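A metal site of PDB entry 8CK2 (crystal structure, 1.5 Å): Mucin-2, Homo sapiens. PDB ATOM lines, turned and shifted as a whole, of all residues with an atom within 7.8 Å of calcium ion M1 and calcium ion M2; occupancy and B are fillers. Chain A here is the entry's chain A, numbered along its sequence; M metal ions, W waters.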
ATOM      1  N   ILE A  10     -20.507  18.052 -33.662  1.00  0.00           N
ATOM      2  CA  ILE A  10     -21.865  18.520 -33.442  1.00  0.00           C
ATOM      3  C   ILE A  10     -22.147  18.436 -31.947  1.00  0.00           C
ATOM      4  O   ILE A  10     -21.988  17.376 -31.343  1.00  0.00           O
ATOM      5  CB  ILE A  10     -22.869  17.669 -34.237  1.00  0.00           C
ATOM      6  CG1 ILE A  10     -22.587  17.753 -35.732  1.00  0.00           C
ATOM      7  CG2 ILE A  10     -24.311  18.121 -33.963  1.00  0.00           C
ATOM      8  CD1 ILE A  10     -23.055  16.532 -36.478  1.00  0.00           C
ATOM      9  N   ASN A  11     -22.582  19.554 -31.357  1.00  0.00           N
ATOM     10  CA  ASN A  11     -22.864  19.571 -29.924  1.00  0.00           C
ATOM     11  C   ASN A  11     -23.943  20.631 -29.695  1.00  0.00           C
ATOM     12  O   ASN A  11     -23.658  21.744 -29.262  1.00  0.00           O
ATOM     13  CB  ASN A  11     -21.619  19.865 -29.071  1.00  0.00           C
ATOM     14  CG  ASN A  11     -21.900  19.713 -27.595  1.00  0.00           C
ATOM     15  OD1 ASN A  11     -22.936  19.156 -27.215  1.00  0.00           O
ATOM     16  ND2 ASN A  11     -20.990  20.213 -26.750  1.00  0.00           N
ATOM     17  N   GLU A  12     -25.191  20.259 -29.999  1.00  0.00           N
ATOM     18  CA  GLU A  12     -26.295  21.207 -29.970  1.00  0.00           C
ATOM     19  C   GLU A  12     -27.177  21.074 -28.744  1.00  0.00           C
ATOM     20  O   GLU A  12     -27.915  22.005 -28.418  1.00  0.00           O
ATOM     21  CB  GLU A  12     -27.175  21.028 -31.213  1.00  0.00           C
ATOM     22  CG  GLU A  12     -26.403  21.341 -32.480  1.00  0.00           C
ATOM     23  CD  GLU A  12     -26.353  22.825 -32.768  1.00  0.00           C
ATOM     24  OE1 GLU A  12     -27.401  23.392 -33.119  1.00  0.00           O
ATOM     25  OE2 GLU A  12     -25.256  23.425 -32.629  1.00  0.00           O
ATOM     26  N   ASP A  13     -27.123  19.932 -28.067  1.00  0.00           N
ATOM     27  CA  ASP A  13     -27.875  19.689 -26.841  1.00  0.00           C
ATOM     28  C   ASP A  13     -26.873  19.611 -25.708  1.00  0.00           C
ATOM     29  O   ASP A  13     -25.664  19.469 -25.951  1.00  0.00           O
ATOM     30  CB  ASP A  13     -28.663  18.372 -26.973  1.00  0.00           C
ATOM     31  CG  ASP A  13     -29.721  18.176 -25.888  1.00  0.00           C
ATOM     32  OD1 ASP A  13     -30.028  19.062 -25.058  1.00  0.00           O
ATOM     33  OD2 ASP A  13     -30.259  17.060 -25.875  1.00  0.00           O
ATOM     34  N   HIS A  14     -27.369  19.693 -24.475  1.00  0.00           N
ATOM     35  CA  HIS A  14     -26.515  19.557 -23.309  1.00  0.00           C
ATOM     36  C   HIS A  14     -27.351  18.967 -22.185  1.00  0.00           C
ATOM     37  O   HIS A  14     -28.572  19.155 -22.170  1.00  0.00           O
ATOM     38  CB  HIS A  14     -25.915  20.911 -22.879  1.00  0.00           C
ATOM     39  CG  HIS A  14     -25.297  21.676 -24.009  1.00  0.00           C
ATOM     40  ND1 HIS A  14     -24.037  21.395 -24.494  1.00  0.00           N
ATOM     41  CD2 HIS A  14     -25.798  22.665 -24.789  1.00  0.00           C
ATOM     42  CE1 HIS A  14     -23.772  22.212 -25.502  1.00  0.00           C
ATOM     43  NE2 HIS A  14     -24.820  22.988 -25.698  1.00  0.00           N
ATOM     44  N   PRO A  15     -26.720  18.266 -21.231  1.00  0.00           N
ATOM     45  CA  PRO A  15     -27.503  17.517 -20.220  1.00  0.00           C
ATOM     46  C   PRO A  15     -28.408  18.356 -19.358  1.00  0.00           C
ATOM     47  O   PRO A  15     -29.369  17.821 -18.820  1.00  0.00           O
ATOM     48  CB  PRO A  15     -26.416  16.868 -19.348  1.00  0.00           C
ATOM     49  CG  PRO A  15     -25.224  16.759 -20.241  1.00  0.00           C
ATOM     50  CD  PRO A  15     -25.278  17.978 -21.139  1.00  0.00           C
ATOM     51  N   SER A  16     -28.097  19.641 -19.152  1.00  0.00           N
ATOM     52  CA  SER A  16     -28.953  20.496 -18.358  1.00  0.00           C
ATOM     53  C   SER A  16     -29.568  21.624 -19.181  1.00  0.00           C
ATOM     54  O   SER A  16     -29.900  22.674 -18.619  1.00  0.00           O
ATOM     55  CB  SER A  16     -28.200  21.067 -17.159  1.00  0.00           C
ATOM     56  OG  SER A  16     -27.580  20.050 -16.389  1.00  0.00           O
ATOM     57  N   SER A  17     -29.703  21.438 -20.486  1.00  0.00           N
ATOM     58  CA  SER A  17     -30.324  22.405 -21.382  1.00  0.00           C
ATOM     59  C   SER A  17     -31.498  21.750 -22.103  1.00  0.00           C
ATOM     60  O   SER A  17     -31.522  20.532 -22.312  1.00  0.00           O
ATOM     61  CB  SER A  17     -29.324  22.953 -22.415  1.00  0.00           C
ATOM     62  OG  SER A  17     -28.074  23.260 -21.830  1.00  0.00           O
ATOM     63  N   GLY A  18     -32.469  22.566 -22.504  1.00  0.00           N
ATOM     64  CA  GLY A  18     -33.620  22.020 -23.193  1.00  0.00           C
ATOM     65  C   GLY A  18     -34.556  21.288 -22.246  1.00  0.00           C
ATOM     66  O   GLY A  18     -34.480  21.390 -21.018  1.00  0.00           O
ATOM     67  N   SER A  19     -35.457  20.507 -22.861  1.00  0.00           N
ATOM     68  CA  SER A  19     -36.557  19.872 -22.157  1.00  0.00           C
ATOM     69  C   SER A  19     -36.479  18.342 -22.152  1.00  0.00           C
ATOM     70  O   SER A  19     -37.416  17.695 -21.666  1.00  0.00           O
ATOM     71  CB  SER A  19     -37.889  20.316 -22.777  1.00  0.00           C
ATOM     72  OG  SER A  19     -37.989  19.885 -24.120  1.00  0.00           O
ATOM     73  N   ASP A  20     -35.388  17.755 -22.653  1.00  0.00           N
ATOM     74  CA  ASP A  20     -35.349  16.319 -22.866  1.00  0.00           C
ATOM     75  C   ASP A  20     -34.712  15.546 -21.720  1.00  0.00           C
ATOM     76  O   ASP A  20     -34.685  14.308 -21.783  1.00  0.00           O
ATOM     77  CB  ASP A  20     -34.645  15.996 -24.204  1.00  0.00           C
ATOM     78  CG  ASP A  20     -33.202  16.528 -24.278  1.00  0.00           C
ATOM     79  OD1 ASP A  20     -32.799  17.411 -23.489  1.00  0.00           O
ATOM     80  OD2 ASP A  20     -32.469  16.045 -25.170  1.00  0.00           O
ATOM     81  N   ASP A  21     -34.235  16.243 -20.685  1.00  0.00           N
ATOM     82  CA  ASP A  21     -33.574  15.595 -19.541  1.00  0.00           C
ATOM     83  C   ASP A  21     -32.524  14.588 -19.986  1.00  0.00           C
ATOM     84  O   ASP A  21     -32.542  13.408 -19.616  1.00  0.00           O
ATOM     85  CB  ASP A  21     -34.604  14.950 -18.619  1.00  0.00           C
ATOM     86  CG  ASP A  21     -33.991  14.514 -17.299  1.00  0.00           C
ATOM     87  OD1 ASP A  21     -33.194  15.284 -16.737  1.00  0.00           O
ATOM     88  OD2 ASP A  21     -34.332  13.395 -16.851  1.00  0.00           O
ATOM     89  N   GLY A  22     -31.624  15.068 -20.839  1.00  0.00           N
ATOM     90  CA  GLY A  22     -30.538  14.234 -21.326  1.00  0.00           C
ATOM     91  C   GLY A  22     -29.760  14.980 -22.383  1.00  0.00           C
ATOM     92  O   GLY A  22     -29.816  16.201 -22.483  1.00  0.00           O
ATOM     93  N   ASP A  23     -29.029  14.219 -23.193  1.00  0.00           N
ATOM     94  CA  ASP A  23     -28.197  14.778 -24.258  1.00  0.00           C
ATOM     95  C   ASP A  23     -28.441  13.964 -25.508  1.00  0.00           C
ATOM     96  O   ASP A  23     -28.148  12.764 -25.540  1.00  0.00           O
ATOM     97  CB  ASP A  23     -26.711  14.764 -23.888  1.00  0.00           C
ATOM     98  CG  ASP A  23     -25.873  15.663 -24.788  1.00  0.00           C
ATOM     99  OD1 ASP A  23     -26.352  16.758 -25.149  1.00  0.00           O
ATOM    100  OD2 ASP A  23     -24.756  15.279 -25.151  1.00  0.00           O
ATOM    101  N   ARG A  24     -29.018  14.599 -26.528  1.00  0.00           N
ATOM    102  CA  ARG A  24     -29.267  13.971 -27.805  1.00  0.00           C
ATOM    103  C   ARG A  24     -28.574  14.775 -28.883  1.00  0.00           C
ATOM    104  O   ARG A  24     -28.660  16.003 -28.914  1.00  0.00           O
ATOM    105  CB  ARG A  24     -30.780  13.867 -28.084  1.00  0.00           C
ATOM    106  CG  ARG A  24     -31.147  13.551 -29.526  1.00  0.00           C
ATOM    107  CD  ARG A  24     -32.233  12.474 -29.602  1.00  0.00           C
ATOM    108  NE  ARG A  24     -32.580  12.095 -30.956  1.00  0.00           N
ATOM    109  CZ  ARG A  24     -31.743  11.547 -31.838  1.00  0.00           C
ATOM    110  NH1 ARG A  24     -30.465  11.322 -31.532  1.00  0.00           N
ATOM    111  NH2 ARG A  24     -32.187  11.218 -33.048  1.00  0.00           N
ATOM    112  N   GLU A  25     -27.854  14.085 -29.763  1.00  0.00           N
ATOM    113  CA  GLU A  25     -27.212  14.733 -30.908  1.00  0.00           C
ATOM    114  C   GLU A  25     -27.622  14.042 -32.192  1.00  0.00           C
ATOM    115  O   GLU A  25     -27.590  12.809 -32.282  1.00  0.00           O
ATOM    116  CB  GLU A  25     -25.681  14.754 -30.794  1.00  0.00           C
ATOM    117  CG  GLU A  25     -25.119  15.426 -29.505  1.00  0.00           C
ATOM    118  CD  GLU A  25     -25.435  16.918 -29.403  1.00  0.00           C
ATOM    119  OE1 GLU A  25     -25.760  17.538 -30.449  1.00  0.00           O
ATOM    120  OE2 GLU A  25     -25.337  17.477 -28.287  1.00  0.00           O
ATOM    121  N   ARG A  40     -18.527  11.080 -28.378  1.00  0.00           N
ATOM    122  CA  ARG A  40     -17.487  11.273 -27.387  1.00  0.00           C
ATOM    123  C   ARG A  40     -17.945  12.259 -26.313  1.00  0.00           C
ATOM    124  O   ARG A  40     -18.656  13.212 -26.608  1.00  0.00           O
ATOM    125  CB  ARG A  40     -16.203  11.821 -28.018  1.00  0.00           C
ATOM    126  CG  ARG A  40     -15.527  10.880 -29.004  1.00  0.00           C
ATOM    127  CD  ARG A  40     -15.000   9.634 -28.316  1.00  0.00           C
ATOM    128  NE  ARG A  40     -14.570   8.629 -29.288  1.00  0.00           N
ATOM    129  CZ  ARG A  40     -13.336   8.526 -29.761  1.00  0.00           C
ATOM    130  NH1 ARG A  40     -12.374   9.349 -29.375  1.00  0.00           N
ATOM    131  NH2 ARG A  40     -13.060   7.590 -30.672  1.00  0.00           N
ATOM    132  N   VAL A  42     -17.498  15.443 -23.959  1.00  0.00           N
ATOM    133  CA  VAL A  42     -16.791  16.704 -24.154  1.00  0.00           C
ATOM    134  C   VAL A  42     -15.585  16.791 -23.236  1.00  0.00           C
ATOM    135  O   VAL A  42     -14.522  17.281 -23.630  1.00  0.00           O
ATOM    136  CB  VAL A  42     -17.752  17.883 -23.968  1.00  0.00           C
ATOM    137  CG1 VAL A  42     -16.980  19.192 -23.862  1.00  0.00           C
ATOM    138  CG2 VAL A  42     -18.766  17.930 -25.108  1.00  0.00           C
ATOM    139  N   PHE A  64     -27.065  10.046 -31.523  1.00  0.00           N
ATOM    140  CA  PHE A  64     -26.660   9.846 -30.137  1.00  0.00           C
ATOM    141  C   PHE A  64     -27.814  10.154 -29.201  1.00  0.00           C
ATOM    142  O   PHE A  64     -28.443  11.208 -29.322  1.00  0.00           O
ATOM    143  CB  PHE A  64     -25.473  10.742 -29.773  1.00  0.00           C
ATOM    144  CG  PHE A  64     -25.048  10.568 -28.349  1.00  0.00           C
ATOM    145  CD1 PHE A  64     -24.248   9.503 -28.006  1.00  0.00           C
ATOM    146  CD2 PHE A  64     -25.482  11.448 -27.363  1.00  0.00           C
ATOM    147  CE1 PHE A  64     -23.884   9.312 -26.700  1.00  0.00           C
ATOM    148  CE2 PHE A  64     -25.120  11.245 -26.045  1.00  0.00           C
ATOM    149  CZ  PHE A  64     -24.325  10.171 -25.711  1.00  0.00           C
ATOM    150  N   CYS A  66     -28.508  10.044 -24.885  1.00  0.00           N
ATOM    151  CA  CYS A  66     -28.284   9.743 -23.474  1.00  0.00           C
ATOM    152  C   CYS A  66     -29.451  10.295 -22.672  1.00  0.00           C
ATOM    153  O   CYS A  66     -29.832  11.453 -22.863  1.00  0.00           O
ATOM    154  CB  CYS A  66     -26.967  10.369 -23.008  1.00  0.00           C
ATOM    155  SG  CYS A  66     -26.501   9.997 -21.281  1.00  0.00           S
ATOM    156  N   ASN A  68     -30.854  11.148 -18.832  1.00  0.00           N
ATOM    157  CA  ASN A  68     -30.231  11.385 -17.521  1.00  0.00           C
ATOM    158  C   ASN A  68     -30.617  10.321 -16.494  1.00  0.00           C
ATOM    159  O   ASN A  68     -29.788   9.931 -15.664  1.00  0.00           O
ATOM    160  CB  ASN A  68     -30.607  12.773 -17.003  1.00  0.00           C
ATOM    161  CG  ASN A  68     -29.850  13.877 -17.707  1.00  0.00           C
ATOM    162  OD1 ASN A  68     -28.785  13.644 -18.274  1.00  0.00           O
ATOM    163  ND2 ASN A  68     -30.396  15.076 -17.675  1.00  0.00           N
ATOM    164  N   TYR A  81     -23.097  12.867 -18.944  1.00  0.00           N
ATOM    165  CA  TYR A  81     -22.065  13.777 -19.430  1.00  0.00           C
ATOM    166  C   TYR A  81     -22.604  14.546 -20.630  1.00  0.00           C
ATOM    167  O   TYR A  81     -23.575  14.141 -21.280  1.00  0.00           O
ATOM    168  CB  TYR A  81     -20.814  13.003 -19.888  1.00  0.00           C
ATOM    169  CG  TYR A  81     -20.148  12.166 -18.827  1.00  0.00           C
ATOM    170  CD1 TYR A  81     -20.062  12.602 -17.523  1.00  0.00           C
ATOM    171  CD2 TYR A  81     -19.617  10.923 -19.156  1.00  0.00           C
ATOM    172  CE1 TYR A  81     -19.424  11.817 -16.547  1.00  0.00           C
ATOM    173  CE2 TYR A  81     -18.989  10.129 -18.198  1.00  0.00           C
ATOM    174  CZ  TYR A  81     -18.902  10.588 -16.904  1.00  0.00           C
ATOM    175  OH  TYR A  81     -18.289   9.803 -15.947  1.00  0.00           O
ATOM    176  N   ASP A  82     -21.942  15.646 -20.981  1.00  0.00           N
ATOM    177  CA  ASP A  82     -22.233  16.287 -22.264  1.00  0.00           C
ATOM    178  C   ASP A  82     -21.454  15.563 -23.344  1.00  0.00           C
ATOM    179  O   ASP A  82     -20.237  15.327 -23.192  1.00  0.00           O
ATOM    180  CB  ASP A  82     -21.856  17.771 -22.251  1.00  0.00           C
ATOM    181  CG  ASP A  82     -22.425  18.526 -23.446  1.00  0.00           C
ATOM    182  OD1 ASP A  82     -23.334  17.988 -24.114  1.00  0.00           O
ATOM    183  OD2 ASP A  82     -21.961  19.648 -23.722  1.00  0.00           O
ATOM    184  N   TYR A  83     -22.139  15.225 -24.443  1.00  0.00           N
ATOM    185  CA  TYR A  83     -21.509  14.490 -25.532  1.00  0.00           C
ATOM    186  C   TYR A  83     -21.579  15.322 -26.810  1.00  0.00           C
ATOM    187  O   TYR A  83     -22.395  16.240 -26.942  1.00  0.00           O
ATOM    188  CB  TYR A  83     -22.190  13.142 -25.787  1.00  0.00           C
ATOM    189  CG  TYR A  83     -22.001  12.150 -24.653  1.00  0.00           C
ATOM    190  CD1 TYR A  83     -22.831  12.183 -23.540  1.00  0.00           C
ATOM    191  CD2 TYR A  83     -21.030  11.158 -24.731  1.00  0.00           C
ATOM    192  CE1 TYR A  83     -22.677  11.286 -22.506  1.00  0.00           C
ATOM    193  CE2 TYR A  83     -20.877  10.239 -23.686  1.00  0.00           C
ATOM    194  CZ  TYR A  83     -21.697  10.327 -22.597  1.00  0.00           C
ATOM    195  OH  TYR A  83     -21.552   9.402 -21.584  1.00  0.00           O
ATOM    196  N   LYS A  84     -20.681  14.968 -27.726  1.00  0.00           N
ATOM    197  CA  LYS A  84     -20.565  15.579 -29.043  1.00  0.00           C
ATOM    198  C   LYS A  84     -20.336  14.462 -30.062  1.00  0.00           C
ATOM    199  O   LYS A  84     -19.833  13.391 -29.713  1.00  0.00           O
ATOM    200  CB  LYS A  84     -19.416  16.587 -29.077  1.00  0.00           C
ATOM    201  CG  LYS A  84     -18.052  15.960 -28.629  1.00  0.00           C
ATOM    202  CD  LYS A  84     -16.916  16.991 -28.676  1.00  0.00           C
ATOM    203  CE  LYS A  84     -15.534  16.327 -28.619  1.00  0.00           C
ATOM    204  NZ  LYS A  84     -14.388  17.306 -28.593  1.00  0.00           N
ATOM    205  N   ILE A  85     -20.735  14.693 -31.316  1.00  0.00           N
ATOM    206  CA  ILE A  85     -20.573  13.648 -32.307  1.00  0.00           C
ATOM    207  C   ILE A  85     -19.936  14.204 -33.580  1.00  0.00           C
ATOM    208  O   ILE A  85     -20.058  15.385 -33.905  1.00  0.00           O
ATOM    209  CB  ILE A  85     -21.900  12.954 -32.677  1.00  0.00           C
ATOM    210  CG1 ILE A  85     -22.854  13.924 -33.398  1.00  0.00           C
ATOM    211  CG2 ILE A  85     -22.560  12.369 -31.428  1.00  0.00           C
ATOM    212  CD1 ILE A  85     -24.084  13.255 -34.059  1.00  0.00           C
HETATM  213 CA    CA M   1     -30.701  18.409 -22.770  1.00  0.00          CA
HETATM  214 CA    CA M   2     -24.295  17.524 -26.274  1.00  0.00          CA
HETATM  215  O   HOH W   1     -31.482  17.990 -20.542  1.00  0.00           O
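The backbone NH (N) of Gly 22 lies close to the side-chain amide nitrogen (ND2) of Asn 68, at 3.4 Å. N of Glu 12 sits at hydrogen-bond distance from OE1 of Glu 25, at 2.8 Å. O of Asp 23 lies within hydrogen-bond range of N of Cys 66 (2.8 Å). The backbone carbonyl oxygen (O) of Asp 82 is in hydrogen-bond range of the backbone NH (N) of Val 42. The side-chain carboxylate (OD2) of Asp 13 sits at hydrogen-bond distance from the backbone NH (N) of Arg 24 (2.8 Å). The backbone carbonyl oxygen (O) of Glu 25 is in hydrogen-bond range of the backbone NH (N) of Phe 64 (2.9 Å). The side-chain carboxylate of Asp 82 sits at hydrogen-bond distance from a ring nitrogen (ND1) of His 14, 2.8 Å away. The side-chain carboxylate of Asp 23 sits close to the backbone NH of His 14 (3.2 Å).
Five residues have an atom within 4 Å of calcium ion M1: Asp 13, His 14, Ser 17, Asp 20 and Gly 22. Along chain A the residues within 4 Å of calcium ion M1 span positions 13 to 22. The nearest printed residue that does not touch calcium ion M1 is Pro 15 (4.1 Å).
Calcium ion M1 is bound by O of Ser 17 (2.3 Å), O of His 14 (2.3 Å), O of Gly 22 (2.4 Å), water W1 (2.4 Å), OD1 of Asp 20 (2.4 Å) and OD1 of Asp 13 (2.5 Å). Calcium ion M1 has six donor atoms within binding distance.
Calcium ion M2 is bound by OE2 of Glu 25, at 2.3 Å. OD1 of Asn 11 is bound to calcium ion M2 (2.3 Å). O of Tyr 83 is bound to calcium ion M2, at 2.4 Å. O of Asp 13 binds calcium ion M2, at 2.4 Å. Calcium ion M2 is bound by the side-chain carboxylate (OD1) of Asp 82 (2.4 Å). OD1 of Asp 23 is bound to calcium ion M2 (2.5 Å). OD2 of Asp 23 is bound to calcium ion M2 (2.6 Å).
Water W1 lies within hydrogen-bond range of the backbone carbonyl oxygen of Pro 15 (2.7 Å), the backbone NH of Gly 22 (2.9 Å) and the backbone NH of Asp 21 (3.3 Å).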
